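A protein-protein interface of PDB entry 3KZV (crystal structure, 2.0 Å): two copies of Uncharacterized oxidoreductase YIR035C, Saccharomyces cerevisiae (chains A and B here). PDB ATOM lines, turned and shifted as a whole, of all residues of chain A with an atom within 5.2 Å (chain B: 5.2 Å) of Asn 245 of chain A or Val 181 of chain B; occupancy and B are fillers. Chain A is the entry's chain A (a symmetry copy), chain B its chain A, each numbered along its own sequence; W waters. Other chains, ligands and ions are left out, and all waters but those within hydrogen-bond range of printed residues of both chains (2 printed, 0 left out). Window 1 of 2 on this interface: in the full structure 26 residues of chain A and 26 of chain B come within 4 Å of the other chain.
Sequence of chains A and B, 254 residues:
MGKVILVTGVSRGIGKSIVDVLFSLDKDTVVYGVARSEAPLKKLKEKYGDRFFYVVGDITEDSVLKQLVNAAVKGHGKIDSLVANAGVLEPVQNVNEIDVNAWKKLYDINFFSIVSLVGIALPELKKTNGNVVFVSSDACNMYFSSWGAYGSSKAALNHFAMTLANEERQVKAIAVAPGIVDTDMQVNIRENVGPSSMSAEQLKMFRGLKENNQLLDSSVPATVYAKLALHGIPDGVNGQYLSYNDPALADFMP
O of Asn 245 of chain A sits close to SD of Met 205 of chain B (3.8 Å).
The side-chain amide nitrogen of Asn 213 of chain B is in hydrogen-bond range of the backbone carbonyl oxygen of Val 181 of chain B, at 3.2 Å.
O of Tyr 244 of chain A touches CE of Met 205 of chain B, at 3.8 Å.
Asn 245 of chain A touches Trp 147 of chain B.
ND2 of Asn 245 of chain A touches CG2 of Val 181 of chain B, 3.6 Å away.
Leu 209 of chain B touches Asn 245 of chain A (CD1 to CB, 3.9 Å).
Asp 246 of chain A touches Met 205 of chain B (O to CE, 3.5 Å).
Trp 147 of chain B touches Pro 247 of chain A.
Met 253 of chain A touches Met 205 of chain B.
Of chain B, only Trp 147, Val 181, Met 205 and Leu 209 come within 4 Å of Asn 245 of chain A.
Of the printed residues of chain B, Met 253 of chain A touches Met 205 (3.5 Å).
Printed residues of chain A within 4 Å of Trp 147 of chain B: Asn 245 and Pro 247.
Printed residues of chain A within 4 Å of Leu 209 of chain B: Asn 245.
The nearest printed residue of chain B that does not touch Asn 245 of chain A is Ile 180 of chain B (5.5 Å).
The nearest printed residue of chain A that does not touch Val 181 of chain B is Tyr 244 of chain A (6.8 Å).
Hydrophobic or aromatic side chains of chain A that line the printed part of chain B: Pro 247 and Met 253.
Among the printed residues, no Asp or Glu carboxylate lies within 4 Å of a Lys or Arg side-chain nitrogen of the other chain.
No position is printed for both chains.
Of the 8 pairs that touch across the chains among the printed residues, none has its exchanged pair printed and touching as well.
Water W2 bridges N of Val 181 of chain B and ND2 of Asn 245 of chain A.
Water W1 bridges the side-chain amide oxygen (OD1) of Asn 245 of chain A (2.9 Å) and the indole nitrogen (NE1) of Trp 147 of chain B (3.1 Å).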
ATOM      1  N   SER A 243      35.884  24.063 -31.616  1.00  0.00           N
ATOM      2  CA  SER A 243      34.587  23.690 -31.020  1.00  0.00           C
ATOM      3  C   SER A 243      33.530  23.531 -32.073  1.00  0.00           C
ATOM      4  O   SER A 243      33.579  24.216 -33.099  1.00  0.00           O
ATOM      5  CB  SER A 243      34.064  24.812 -30.099  1.00  0.00           C
ATOM      6  OG  SER A 243      35.162  25.243 -29.329  1.00  0.00           O
ATOM      7  N   TYR A 244      32.534  22.684 -31.769  1.00  0.00           N
ATOM      8  CA  TYR A 244      31.469  22.354 -32.703  1.00  0.00           C
ATOM      9  C   TYR A 244      30.714  23.641 -33.005  1.00  0.00           C
ATOM     10  O   TYR A 244      30.138  23.756 -34.093  1.00  0.00           O
ATOM     11  CB  TYR A 244      30.511  21.332 -32.089  1.00  0.00           C
ATOM     12  CG  TYR A 244      29.522  21.976 -31.130  1.00  0.00           C
ATOM     13  CD1 TYR A 244      28.220  22.294 -31.553  1.00  0.00           C
ATOM     14  CD2 TYR A 244      29.890  22.328 -29.861  1.00  0.00           C
ATOM     15  CE1 TYR A 244      27.335  22.924 -30.704  1.00  0.00           C
ATOM     16  CE2 TYR A 244      28.969  22.975 -28.966  1.00  0.00           C
ATOM     17  CZ  TYR A 244      27.702  23.232 -29.415  1.00  0.00           C
ATOM     18  OH  TYR A 244      26.813  23.859 -28.616  1.00  0.00           O
ATOM     19  N   ASN A 245      30.778  24.608 -32.075  1.00  0.00           N
ATOM     20  CA  ASN A 245      30.064  25.863 -32.233  1.00  0.00           C
ATOM     21  C   ASN A 245      30.970  27.003 -32.741  1.00  0.00           C
ATOM     22  O   ASN A 245      30.624  28.168 -32.557  1.00  0.00           O
ATOM     23  CB  ASN A 245      29.322  26.297 -30.951  1.00  0.00           C
ATOM     24  CG  ASN A 245      30.226  26.409 -29.746  1.00  0.00           C
ATOM     25  OD1 ASN A 245      31.434  26.369 -29.880  1.00  0.00           O
ATOM     26  ND2 ASN A 245      29.638  26.653 -28.561  1.00  0.00           N
ATOM     27  N   ASP A 246      32.095  26.689 -33.393  1.00  0.00           N
ATOM     28  CA  ASP A 246      32.856  27.782 -34.017  1.00  0.00           C
ATOM     29  C   ASP A 246      32.092  28.269 -35.281  1.00  0.00           C
ATOM     30  O   ASP A 246      31.552  27.452 -36.059  1.00  0.00           O
ATOM     31  CB  ASP A 246      34.271  27.355 -34.392  1.00  0.00           C
ATOM     32  CG  ASP A 246      35.072  28.504 -34.924  1.00  0.00           C
ATOM     33  OD1 ASP A 246      35.479  29.391 -34.122  1.00  0.00           O
ATOM     34  OD2 ASP A 246      35.082  28.594 -36.159  1.00  0.00           O
ATOM     35  N   PRO A 247      32.040  29.574 -35.524  1.00  0.00           N
ATOM     36  CA  PRO A 247      31.248  29.999 -36.675  1.00  0.00           C
ATOM     37  C   PRO A 247      31.670  29.375 -38.023  1.00  0.00           C
ATOM     38  O   PRO A 247      30.847  29.246 -38.921  1.00  0.00           O
ATOM     39  CB  PRO A 247      31.463  31.509 -36.706  1.00  0.00           C
ATOM     40  CG  PRO A 247      31.550  31.888 -35.253  1.00  0.00           C
ATOM     41  CD  PRO A 247      32.389  30.718 -34.650  1.00  0.00           C
ATOM     42  N   MET A 253      25.691  22.786 -38.703  1.00  0.00           N
ATOM     43  CA  MET A 253      24.702  22.730 -37.618  1.00  0.00           C
ATOM     44  C   MET A 253      23.368  22.117 -38.153  1.00  0.00           C
ATOM     45  O   MET A 253      23.163  22.071 -39.365  1.00  0.00           O
ATOM     46  CB  MET A 253      24.446  24.157 -37.075  1.00  0.00           C
ATOM     47  CG  MET A 253      25.617  24.694 -36.213  1.00  0.00           C
ATOM     48  SD  MET A 253      25.828  24.008 -34.554  1.00  0.00           S
ATOM     49  CE  MET A 253      24.339  24.801 -33.803  1.00  0.00           C
ATOM     50  N   LEU B  89      26.597  37.624 -25.060  1.00  0.00           N
ATOM     51  CA  LEU B  89      26.961  37.996 -26.424  1.00  0.00           C
ATOM     52  C   LEU B  89      25.805  38.692 -27.172  1.00  0.00           C
ATOM     53  O   LEU B  89      24.695  38.207 -27.120  1.00  0.00           O
ATOM     54  CB  LEU B  89      27.366  36.709 -27.160  1.00  0.00           C
ATOM     55  CG  LEU B  89      27.629  36.855 -28.645  1.00  0.00           C
ATOM     56  CD1 LEU B  89      28.763  37.850 -28.857  1.00  0.00           C
ATOM     57  CD2 LEU B  89      27.888  35.557 -29.223  1.00  0.00           C
ATOM     58  N   TRP B 147      35.238  33.764 -34.084  1.00  0.00           N
ATOM     59  CA  TRP B 147      34.388  34.795 -33.475  1.00  0.00           C
ATOM     60  C   TRP B 147      35.007  36.211 -33.514  1.00  0.00           C
ATOM     61  O   TRP B 147      34.430  37.141 -32.937  1.00  0.00           O
ATOM     62  CB  TRP B 147      34.123  34.474 -32.031  1.00  0.00           C
ATOM     63  CG  TRP B 147      33.084  33.420 -31.840  1.00  0.00           C
ATOM     64  CD1 TRP B 147      33.295  32.188 -31.320  1.00  0.00           C
ATOM     65  CD2 TRP B 147      31.699  33.517 -32.113  1.00  0.00           C
ATOM     66  NE1 TRP B 147      32.121  31.485 -31.250  1.00  0.00           N
ATOM     67  CE2 TRP B 147      31.115  32.281 -31.729  1.00  0.00           C
ATOM     68  CE3 TRP B 147      30.872  34.526 -32.681  1.00  0.00           C
ATOM     69  CZ2 TRP B 147      29.737  31.999 -31.896  1.00  0.00           C
ATOM     70  CZ3 TRP B 147      29.492  34.255 -32.837  1.00  0.00           C
ATOM     71  CH2 TRP B 147      28.945  32.985 -32.440  1.00  0.00           C
ATOM     72  N   GLY B 179      31.021  26.709 -20.069  1.00  0.00           N
ATOM     73  CA  GLY B 179      30.684  25.470 -20.843  1.00  0.00           C
ATOM     74  C   GLY B 179      29.614  25.729 -21.902  1.00  0.00           C
ATOM     75  O   GLY B 179      28.987  24.766 -22.397  1.00  0.00           O
ATOM     76  N   ILE B 180      29.322  27.018 -22.144  1.00  0.00           N
ATOM     77  CA  ILE B 180      28.320  27.487 -23.150  1.00  0.00           C
ATOM     78  C   ILE B 180      28.756  28.864 -23.630  1.00  0.00           C
ATOM     79  O   ILE B 180      29.622  29.520 -22.998  1.00  0.00           O
ATOM     80  CB  ILE B 180      26.864  27.619 -22.606  1.00  0.00           C
ATOM     81  CG1 ILE B 180      26.827  28.534 -21.378  1.00  0.00           C
ATOM     82  CG2 ILE B 180      26.227  26.207 -22.334  1.00  0.00           C
ATOM     83  CD1 ILE B 180      25.458  29.036 -20.983  1.00  0.00           C
ATOM     84  N   VAL B 181      28.201  29.303 -24.765  1.00  0.00           N
ATOM     85  CA  VAL B 181      28.374  30.679 -25.188  1.00  0.00           C
ATOM     86  C   VAL B 181      27.233  31.411 -24.507  1.00  0.00           C
ATOM     87  O   VAL B 181      26.079  31.054 -24.696  1.00  0.00           O
ATOM     88  CB  VAL B 181      28.316  30.838 -26.729  1.00  0.00           C
ATOM     89  CG1 VAL B 181      28.341  32.338 -27.106  1.00  0.00           C
ATOM     90  CG2 VAL B 181      29.562  30.098 -27.405  1.00  0.00           C
ATOM     91  N   ASP B 182      27.543  32.402 -23.677  1.00  0.00           N
ATOM     92  CA  ASP B 182      26.522  33.105 -22.856  1.00  0.00           C
ATOM     93  C   ASP B 182      25.618  33.964 -23.758  1.00  0.00           C
ATOM     94  O   ASP B 182      26.067  34.955 -24.369  1.00  0.00           O
ATOM     95  CB  ASP B 182      27.218  33.989 -21.801  1.00  0.00           C
ATOM     96  CG  ASP B 182      26.226  34.615 -20.779  1.00  0.00           C
ATOM     97  OD1 ASP B 182      25.157  34.036 -20.492  1.00  0.00           O
ATOM     98  OD2 ASP B 182      26.502  35.743 -20.307  1.00  0.00           O
ATOM     99  N   THR B 183      24.353  33.568 -23.867  1.00  0.00           N
ATOM    100  CA  THR B 183      23.383  34.297 -24.666  1.00  0.00           C
ATOM    101  C   THR B 183      22.093  34.528 -23.874  1.00  0.00           C
ATOM    102  O   THR B 183      21.845  33.930 -22.800  1.00  0.00           O
ATOM    103  CB  THR B 183      23.035  33.586 -26.009  1.00  0.00           C
ATOM    104  OG1 THR B 183      22.296  32.397 -25.714  1.00  0.00           O
ATOM    105  CG2 THR B 183      24.309  33.211 -26.833  1.00  0.00           C
ATOM    106  N   MET B 205      25.519  31.041 -36.561  1.00  0.00           N
ATOM    107  CA  MET B 205      25.861  30.254 -35.329  1.00  0.00           C
ATOM    108  C   MET B 205      25.218  30.877 -34.093  1.00  0.00           C
ATOM    109  O   MET B 205      24.644  30.193 -33.219  1.00  0.00           O
ATOM    110  CB  MET B 205      27.406  30.162 -35.129  1.00  0.00           C
ATOM    111  CG  MET B 205      27.783  29.288 -33.806  1.00  0.00           C
ATOM    112  SD  MET B 205      27.173  27.536 -33.966  1.00  0.00           S
ATOM    113  CE  MET B 205      28.243  26.858 -35.241  1.00  0.00           C
ATOM    114  N   LEU B 209      22.825  28.959 -31.574  1.00  0.00           N
ATOM    115  CA  LEU B 209      23.134  28.813 -30.175  1.00  0.00           C
ATOM    116  C   LEU B 209      22.019  29.362 -29.323  1.00  0.00           C
ATOM    117  O   LEU B 209      21.597  28.743 -28.385  1.00  0.00           O
ATOM    118  CB  LEU B 209      24.418  29.541 -29.841  1.00  0.00           C
ATOM    119  CG  LEU B 209      25.730  28.782 -29.736  1.00  0.00           C
ATOM    120  CD1 LEU B 209      25.697  27.496 -30.453  1.00  0.00           C
ATOM    121  CD2 LEU B 209      26.841  29.585 -30.194  1.00  0.00           C
ATOM    122  N   ASN B 213      19.818  27.527 -26.362  1.00  0.00           N
ATOM    123  CA  ASN B 213      20.016  27.752 -24.935  1.00  0.00           C
ATOM    124  C   ASN B 213      18.698  27.946 -24.193  1.00  0.00           C
ATOM    125  O   ASN B 213      17.754  28.531 -24.726  1.00  0.00           O
ATOM    126  CB  ASN B 213      20.931  28.957 -24.704  1.00  0.00           C
ATOM    127  CG  ASN B 213      22.401  28.588 -24.741  1.00  0.00           C
ATOM    128  OD1 ASN B 213      22.774  27.450 -24.458  1.00  0.00           O
ATOM    129  ND2 ASN B 213      23.244  29.552 -25.091  1.00  0.00           N
HETATM  130  O   HOH W   1      33.027  28.781 -30.019  1.00  0.00           O
HETATM  131  O   HOH W   2      27.055  27.383 -26.558  1.00  0.00           O
